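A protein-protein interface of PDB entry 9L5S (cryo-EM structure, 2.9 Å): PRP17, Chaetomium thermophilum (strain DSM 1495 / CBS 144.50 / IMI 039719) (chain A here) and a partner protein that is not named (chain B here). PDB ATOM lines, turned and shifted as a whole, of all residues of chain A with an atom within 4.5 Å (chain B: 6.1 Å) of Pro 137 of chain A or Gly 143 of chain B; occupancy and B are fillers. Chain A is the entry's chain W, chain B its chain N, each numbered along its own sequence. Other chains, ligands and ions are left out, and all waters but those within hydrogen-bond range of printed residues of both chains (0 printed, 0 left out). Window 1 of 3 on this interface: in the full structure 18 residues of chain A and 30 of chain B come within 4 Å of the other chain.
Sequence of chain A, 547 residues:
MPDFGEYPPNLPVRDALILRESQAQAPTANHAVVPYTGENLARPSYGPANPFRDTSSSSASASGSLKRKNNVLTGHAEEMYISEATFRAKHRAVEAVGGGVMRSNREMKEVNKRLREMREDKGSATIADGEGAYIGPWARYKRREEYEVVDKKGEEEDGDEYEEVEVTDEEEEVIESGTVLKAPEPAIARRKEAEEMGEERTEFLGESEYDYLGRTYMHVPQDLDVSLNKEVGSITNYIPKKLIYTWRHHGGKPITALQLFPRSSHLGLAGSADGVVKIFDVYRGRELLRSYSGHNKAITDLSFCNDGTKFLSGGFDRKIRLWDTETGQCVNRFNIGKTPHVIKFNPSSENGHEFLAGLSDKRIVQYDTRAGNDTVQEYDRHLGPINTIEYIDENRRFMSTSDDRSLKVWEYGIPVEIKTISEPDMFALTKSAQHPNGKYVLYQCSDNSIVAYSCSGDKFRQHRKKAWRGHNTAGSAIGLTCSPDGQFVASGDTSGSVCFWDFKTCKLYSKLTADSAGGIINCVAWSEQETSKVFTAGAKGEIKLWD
The side-chain hydroxyl (OH) of Tyr 134 of chain A is in hydrogen-bond range of a ring nitrogen (NE2) of His 56 of chain B. NH2 of Arg 119 of chain A sits at hydrogen-bond distance from O of Arg 142 of chain B. N of Arg 142 of chain B lies within hydrogen-bond range of O of Pro 137 of chain A. The backbone carbonyl oxygen of Trp 138 of chain A lies within hydrogen-bond range of the guanidinium group of Arg 142 of chain B. The backbone carbonyl oxygen (O) of Gly 143 of chain B lies within hydrogen-bond range of the guanidinium group (NH2) of Arg 119 of chain A, at 2.9 Å. NH1 of Arg 119 of chain A lies within salt-bridge range of OXT of Asp 148 of chain B, at 3.2 Å. The backbone NH (N) of Cys 141 of chain B sits close to the indole nitrogen (NE1) of Trp 138 of chain A, at 3.5 Å.
ND1 of His 56 of chain B sits close to O of Leu 102 of chain B, 3.4 Å away. NZ of Lys 101 of chain B is in salt-bridge range of O of Asp 148 of chain B (2.4 Å). The backbone carbonyl oxygen of Cys 144 of chain B sits at hydrogen-bond distance from the guanidinium group of Arg 122 of chain B (3.1 Å). The side-chain sulfur (SG) of Cys 141 of chain B lies close to the backbone NH (N) of Gly 143 of chain B (3.3 Å). The guanidinium group (NH2) of Arg 119 of chain A is in hydrogen-bond range of the backbone carbonyl oxygen (O) of Pro 137 of chain A (2.9 Å). The guanidinium group of Arg 119 of chain A lies within hydrogen-bond range of the backbone carbonyl oxygen of Ala 139 of chain A, at 2.6 Å.
Among the printed residues, pairs that only touch across the chains: Trp 138 of chain A with Gly 140 of chain B, Pro 137 of chain A with Lys 101 of chain B, Trp 138 of chain A with His 56 of chain B, Pro 137 of chain A with Cys 141 of chain B, Ala 139 of chain A with Arg 142 of chain B, Pro 137 of chain A with Gly 143 of chain B, Pro 137 of chain A with Cys 144 of chain B, Pro 137 of chain A with His 56 of chain B and Trp 138 of chain A with Cys 103 of chain B.
Of the printed residues of chain B, Tyr 134 of chain A touches His 56. Pro 137 of chain A touches just these residues of chain B: His 56 (3.8 Å), Lys 101 (3.4 Å), Cys 141 (3.6 Å), Arg 142 (3.0 Å), Gly 143 (3.7 Å) and Cys 144 (3.7 Å). Printed residues of chain B within 4 Å of Trp 138 of chain A: His 56, Cys 103, Gly 140, Cys 141 and Arg 142. Of the printed residues of chain A, Gly 140 of chain B touches Trp 138. Gly 143 of chain B touches just these residues of chain A: Arg 119 and Pro 137. The nearest residue of chain B that does not touch Pro 137 of chain A is Cys 103 of chain B (4.2 Å).
Of the 16 printed residues of chain B, 9 touch a printed residue of chain A. Hydrophobic or aromatic side chains of chain A that line the printed part of chain B: Tyr 134, Pro 137 and Trp 138. Among the printed residues, no Asp or Glu carboxylate lies within 4 Å of a Lys or Arg side-chain nitrogen of the other chain.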
ATOM      1  N   ARG A 119      -1.334   7.352  20.007  1.00  0.00           N
ATOM      2  CA  ARG A 119      -2.301   7.356  21.094  1.00  0.00           C
ATOM      3  C   ARG A 119      -2.535   8.776  21.615  1.00  0.00           C
ATOM      4  O   ARG A 119      -1.777   9.707  21.330  1.00  0.00           O
ATOM      5  CB  ARG A 119      -1.810   6.452  22.225  1.00  0.00           C
ATOM      6  CG  ARG A 119      -2.889   5.754  23.034  1.00  0.00           C
ATOM      7  CD  ARG A 119      -2.281   5.127  24.276  1.00  0.00           C
ATOM      8  NE  ARG A 119      -3.220   4.270  24.989  1.00  0.00           N
ATOM      9  CZ  ARG A 119      -2.869   3.394  25.919  1.00  0.00           C
ATOM     10  NH1 ARG A 119      -1.606   3.240  26.280  1.00  0.00           N
ATOM     11  NH2 ARG A 119      -3.806   2.653  26.500  1.00  0.00           N
ATOM     12  N   TYR A 134      -5.196  13.188  34.423  1.00  0.00           N
ATOM     13  CA  TYR A 134      -4.589  11.902  34.110  1.00  0.00           C
ATOM     14  C   TYR A 134      -5.636  10.933  33.581  1.00  0.00           C
ATOM     15  O   TYR A 134      -6.641  10.661  34.248  1.00  0.00           O
ATOM     16  CB  TYR A 134      -3.920  11.326  35.350  1.00  0.00           C
ATOM     17  CG  TYR A 134      -3.170  10.042  35.100  1.00  0.00           C
ATOM     18  CD1 TYR A 134      -2.055  10.018  34.274  1.00  0.00           C
ATOM     19  CD2 TYR A 134      -3.575   8.855  35.691  1.00  0.00           C
ATOM     20  CE1 TYR A 134      -1.363   8.845  34.045  1.00  0.00           C
ATOM     21  CE2 TYR A 134      -2.893   7.681  35.467  1.00  0.00           C
ATOM     22  CZ  TYR A 134      -1.788   7.680  34.646  1.00  0.00           C
ATOM     23  OH  TYR A 134      -1.107   6.506  34.420  1.00  0.00           O
ATOM     24  N   ILE A 135      -5.395  10.405  32.386  1.00  0.00           N
ATOM     25  CA  ILE A 135      -6.240   9.376  31.803  1.00  0.00           C
ATOM     26  C   ILE A 135      -5.558   8.014  31.845  1.00  0.00           C
ATOM     27  O   ILE A 135      -6.173   7.020  32.234  1.00  0.00           O
ATOM     28  CB  ILE A 135      -6.630   9.781  30.364  1.00  0.00           C
ATOM     29  CG1 ILE A 135      -7.778  10.790  30.402  1.00  0.00           C
ATOM     30  CG2 ILE A 135      -7.056   8.581  29.550  1.00  0.00           C
ATOM     31  CD1 ILE A 135      -8.226  11.266  29.038  1.00  0.00           C
ATOM     32  N   GLY A 136      -4.279   7.961  31.482  1.00  0.00           N
ATOM     33  CA  GLY A 136      -3.464   6.791  31.701  1.00  0.00           C
ATOM     34  C   GLY A 136      -3.710   5.670  30.718  1.00  0.00           C
ATOM     35  O   GLY A 136      -3.859   5.886  29.511  1.00  0.00           O
ATOM     36  N   PRO A 137      -3.745   4.432  31.224  1.00  0.00           N
ATOM     37  CA  PRO A 137      -3.947   3.269  30.343  1.00  0.00           C
ATOM     38  C   PRO A 137      -5.318   3.216  29.685  1.00  0.00           C
ATOM     39  O   PRO A 137      -5.516   2.396  28.780  1.00  0.00           O
ATOM     40  CB  PRO A 137      -3.748   2.076  31.285  1.00  0.00           C
ATOM     41  CG  PRO A 137      -3.024   2.602  32.461  1.00  0.00           C
ATOM     42  CD  PRO A 137      -3.386   4.041  32.596  1.00  0.00           C
ATOM     43  N   TRP A 138      -6.259   4.055  30.105  1.00  0.00           N
ATOM     44  CA  TRP A 138      -7.562   4.185  29.475  1.00  0.00           C
ATOM     45  C   TRP A 138      -7.558   5.179  28.321  1.00  0.00           C
ATOM     46  O   TRP A 138      -8.630   5.536  27.821  1.00  0.00           O
ATOM     47  CB  TRP A 138      -8.601   4.575  30.528  1.00  0.00           C
ATOM     48  CG  TRP A 138      -8.801   3.498  31.550  1.00  0.00           C
ATOM     49  CD1 TRP A 138      -9.703   2.484  31.491  1.00  0.00           C
ATOM     50  CD2 TRP A 138      -8.030   3.279  32.738  1.00  0.00           C
ATOM     51  NE1 TRP A 138      -9.578   1.669  32.586  1.00  0.00           N
ATOM     52  CE2 TRP A 138      -8.553   2.133  33.367  1.00  0.00           C
ATOM     53  CE3 TRP A 138      -6.964   3.950  33.342  1.00  0.00           C
ATOM     54  CZ2 TRP A 138      -8.047   1.643  34.567  1.00  0.00           C
ATOM     55  CZ3 TRP A 138      -6.462   3.463  34.531  1.00  0.00           C
ATOM     56  CH2 TRP A 138      -7.003   2.319  35.130  1.00  0.00           C
ATOM     57  N   ALA A 139      -6.383   5.632  27.893  1.00  0.00           N
ATOM     58  CA  ALA A 139      -6.283   6.424  26.676  1.00  0.00           C
ATOM     59  C   ALA A 139      -6.444   5.528  25.457  1.00  0.00           C
ATOM     60  O   ALA A 139      -5.785   4.493  25.333  1.00  0.00           O
ATOM     61  CB  ALA A 139      -4.942   7.154  26.623  1.00  0.00           C
ATOM     62  N   HIS B  56      -6.985   4.176  40.251  1.00  0.00           N
ATOM     63  CA  HIS B  56      -5.701   4.350  39.578  1.00  0.00           C
ATOM     64  C   HIS B  56      -5.285   5.815  39.547  1.00  0.00           C
ATOM     65  O   HIS B  56      -4.120   6.133  39.801  1.00  0.00           O
ATOM     66  CB  HIS B  56      -5.787   3.781  38.159  1.00  0.00           C
ATOM     67  CG  HIS B  56      -4.492   3.793  37.402  1.00  0.00           C
ATOM     68  ND1 HIS B  56      -3.920   2.646  36.900  1.00  0.00           N
ATOM     69  CD2 HIS B  56      -3.688   4.811  37.015  1.00  0.00           C
ATOM     70  CE1 HIS B  56      -2.804   2.954  36.263  1.00  0.00           C
ATOM     71  NE2 HIS B  56      -2.638   4.262  36.322  1.00  0.00           N
ATOM     72  N   LYS B 101       3.173   1.243  34.453  1.00  0.00           N
ATOM     73  CA  LYS B 101       1.915   1.827  34.008  1.00  0.00           C
ATOM     74  C   LYS B 101       0.749   0.864  34.179  1.00  0.00           C
ATOM     75  O   LYS B 101      -0.256   0.992  33.477  1.00  0.00           O
ATOM     76  CB  LYS B 101       2.022   2.278  32.550  1.00  0.00           C
ATOM     77  CG  LYS B 101       3.154   3.258  32.286  1.00  0.00           C
ATOM     78  CD  LYS B 101       3.545   3.271  30.819  1.00  0.00           C
ATOM     79  CE  LYS B 101       3.998   4.653  30.379  1.00  0.00           C
ATOM     80  NZ  LYS B 101       4.465   4.658  28.965  1.00  0.00           N
ATOM     81  N   LEU B 102       0.875  -0.101  35.090  1.00  0.00           N
ATOM     82  CA  LEU B 102      -0.142  -1.130  35.271  1.00  0.00           C
ATOM     83  C   LEU B 102      -1.461  -0.529  35.740  1.00  0.00           C
ATOM     84  O   LEU B 102      -1.498   0.252  36.693  1.00  0.00           O
ATOM     85  CB  LEU B 102       0.348  -2.172  36.275  1.00  0.00           C
ATOM     86  CG  LEU B 102      -0.701  -3.145  36.809  1.00  0.00           C
ATOM     87  CD1 LEU B 102      -1.031  -4.185  35.768  1.00  0.00           C
ATOM     88  CD2 LEU B 102      -0.214  -3.803  38.083  1.00  0.00           C
ATOM     89  N   CYS B 103      -2.546  -0.914  35.060  1.00  0.00           N
ATOM     90  CA  CYS B 103      -3.862  -0.340  35.325  1.00  0.00           C
ATOM     91  C   CYS B 103      -4.371  -0.712  36.711  1.00  0.00           C
ATOM     92  O   CYS B 103      -4.776   0.158  37.490  1.00  0.00           O
ATOM     93  CB  CYS B 103      -4.844  -0.808  34.255  1.00  0.00           C
ATOM     94  SG  CYS B 103      -4.904  -2.605  34.080  1.00  0.00           S
ATOM     95  N   ILE B 120      -5.081  -9.261  28.569  1.00  0.00           N
ATOM     96  CA  ILE B 120      -4.652  -8.902  27.223  1.00  0.00           C
ATOM     97  C   ILE B 120      -4.172  -7.456  27.151  1.00  0.00           C
ATOM     98  O   ILE B 120      -3.462  -7.089  26.208  1.00  0.00           O
ATOM     99  CB  ILE B 120      -5.793  -9.181  26.222  1.00  0.00           C
ATOM    100  CG1 ILE B 120      -5.245  -9.385  24.806  1.00  0.00           C
ATOM    101  CG2 ILE B 120      -6.843  -8.076  26.255  1.00  0.00           C
ATOM    102  CD1 ILE B 120      -6.272  -9.895  23.827  1.00  0.00           C
ATOM    103  N   CYS B 121      -4.525  -6.622  28.132  1.00  0.00           N
ATOM    104  CA  CYS B 121      -4.044  -5.249  28.183  1.00  0.00           C
ATOM    105  C   CYS B 121      -2.602  -5.141  28.662  1.00  0.00           C
ATOM    106  O   CYS B 121      -2.000  -4.071  28.524  1.00  0.00           O
ATOM    107  CB  CYS B 121      -4.970  -4.404  29.066  1.00  0.00           C
ATOM    108  SG  CYS B 121      -4.932  -4.767  30.834  1.00  0.00           S
ATOM    109  N   ARG B 122      -2.031  -6.213  29.212  1.00  0.00           N
ATOM    110  CA  ARG B 122      -0.619  -6.231  29.567  1.00  0.00           C
ATOM    111  C   ARG B 122       0.293  -6.379  28.358  1.00  0.00           C
ATOM    112  O   ARG B 122       1.501  -6.149  28.481  1.00  0.00           O
ATOM    113  CB  ARG B 122      -0.331  -7.372  30.544  1.00  0.00           C
ATOM    114  CG  ARG B 122      -0.980  -7.224  31.902  1.00  0.00           C
ATOM    115  CD  ARG B 122      -0.480  -5.979  32.596  1.00  0.00           C
ATOM    116  NE  ARG B 122       0.933  -6.065  32.941  1.00  0.00           N
ATOM    117  CZ  ARG B 122       1.742  -5.020  33.038  1.00  0.00           C
ATOM    118  NH1 ARG B 122       1.309  -3.790  32.825  1.00  0.00           N
ATOM    119  NH2 ARG B 122       3.018  -5.214  33.354  1.00  0.00           N
ATOM    120  N   VAL B 123      -0.253  -6.757  27.209  1.00  0.00           N
ATOM    121  CA  VAL B 123       0.516  -7.056  26.004  1.00  0.00           C
ATOM    122  C   VAL B 123       0.962  -5.753  25.350  1.00  0.00           C
ATOM    123  O   VAL B 123       0.181  -4.792  25.302  1.00  0.00           O
ATOM    124  CB  VAL B 123      -0.318  -7.917  25.041  1.00  0.00           C
ATOM    125  CG1 VAL B 123       0.465  -8.276  23.788  1.00  0.00           C
ATOM    126  CG2 VAL B 123      -0.797  -9.161  25.752  1.00  0.00           C
ATOM    127  N   ILE B 134      -8.717  -3.013  21.966  1.00  0.00           N
ATOM    128  CA  ILE B 134      -9.068  -3.869  23.088  1.00  0.00           C
ATOM    129  C   ILE B 134      -9.521  -3.003  24.255  1.00  0.00           C
ATOM    130  O   ILE B 134      -9.106  -1.846  24.406  1.00  0.00           O
ATOM    131  CB  ILE B 134      -7.890  -4.778  23.492  1.00  0.00           C
ATOM    132  CG1 ILE B 134      -6.716  -3.953  24.025  1.00  0.00           C
ATOM    133  CG2 ILE B 134      -7.455  -5.645  22.326  1.00  0.00           C
ATOM    134  CD1 ILE B 134      -5.710  -4.758  24.812  1.00  0.00           C
ATOM    135  N   GLY B 140     -11.532  -1.952  31.853  1.00  0.00           N
ATOM    136  CA  GLY B 140     -11.624  -1.061  30.713  1.00  0.00           C
ATOM    137  C   GLY B 140     -10.303  -0.564  30.186  1.00  0.00           C
ATOM    138  O   GLY B 140     -10.288   0.361  29.368  1.00  0.00           O
ATOM    139  N   CYS B 141      -9.194  -1.157  30.621  1.00  0.00           N
ATOM    140  CA  CYS B 141      -7.873  -0.734  30.180  1.00  0.00           C
ATOM    141  C   CYS B 141      -7.680  -1.007  28.694  1.00  0.00           C
ATOM    142  O   CYS B 141      -8.048  -2.067  28.184  1.00  0.00           O
ATOM    143  CB  CYS B 141      -6.795  -1.453  30.986  1.00  0.00           C
ATOM    144  SG  CYS B 141      -5.108  -1.109  30.466  1.00  0.00           S
ATOM    145  N   ARG B 142      -7.096  -0.032  28.003  1.00  0.00           N
ATOM    146  CA  ARG B 142      -6.846  -0.105  26.572  1.00  0.00           C
ATOM    147  C   ARG B 142      -5.394  -0.426  26.252  1.00  0.00           C
ATOM    148  O   ARG B 142      -4.945  -0.182  25.128  1.00  0.00           O
ATOM    149  CB  ARG B 142      -7.278   1.204  25.911  1.00  0.00           C
ATOM    150  CG  ARG B 142      -8.762   1.232  25.609  1.00  0.00           C
ATOM    151  CD  ARG B 142      -9.320   2.635  25.574  1.00  0.00           C
ATOM    152  NE  ARG B 142     -10.645   2.663  24.967  1.00  0.00           N
ATOM    153  CZ  ARG B 142     -11.572   3.572  25.233  1.00  0.00           C
ATOM    154  NH1 ARG B 142     -11.371   4.521  26.132  1.00  0.00           N
ATOM    155  NH2 ARG B 142     -12.734   3.521  24.588  1.00  0.00           N
ATOM    156  N   GLY B 143      -4.660  -0.972  27.215  1.00  0.00           N
ATOM    157  CA  GLY B 143      -3.253  -1.275  27.067  1.00  0.00           C
ATOM    158  C   GLY B 143      -2.424  -0.550  28.104  1.00  0.00           C
ATOM    159  O   GLY B 143      -2.347   0.681  28.104  1.00  0.00           O
ATOM    160  N   CYS B 144      -1.794  -1.313  28.998  1.00  0.00           N
ATOM    161  CA  CYS B 144      -1.029  -0.754  30.105  1.00  0.00           C
ATOM    162  C   CYS B 144       0.403  -1.274  30.129  1.00  0.00           C
ATOM    163  O   CYS B 144       1.055  -1.231  31.176  1.00  0.00           O
ATOM    164  CB  CYS B 144      -1.717  -1.051  31.436  1.00  0.00           C
ATOM    165  SG  CYS B 144      -1.951  -2.799  31.774  1.00  0.00           S
ATOM    166  N   ALA B 145       0.889  -1.791  29.004  1.00  0.00           N
ATOM    167  CA  ALA B 145       2.287  -2.175  28.903  1.00  0.00           C
ATOM    168  C   ALA B 145       3.173  -0.942  29.030  1.00  0.00           C
ATOM    169  O   ALA B 145       2.782   0.169  28.663  1.00  0.00           O
ATOM    170  CB  ALA B 145       2.555  -2.888  27.578  1.00  0.00           C
ATOM    171  N   ASP B 148       3.931   1.155  26.056  1.00  0.00           N
ATOM    172  CA  ASP B 148       2.800   1.889  25.501  1.00  0.00           C
ATOM    173  C   ASP B 148       2.593   3.212  26.229  1.00  0.00           C
ATOM    174  O   ASP B 148       3.447   3.656  26.996  1.00  0.00           O
ATOM    175  CB  ASP B 148       1.525   1.047  25.572  1.00  0.00           C
ATOM    176  CG  ASP B 148       1.673  -0.290  24.876  1.00  0.00           C
ATOM    177  OD1 ASP B 148       2.697  -0.492  24.190  1.00  0.00           O
ATOM    178  OD2 ASP B 148       0.765  -1.136  25.012  1.00  0.00           O
ATOM    179  OXT ASP B 148       1.567   3.872  26.065  1.00  0.00           O
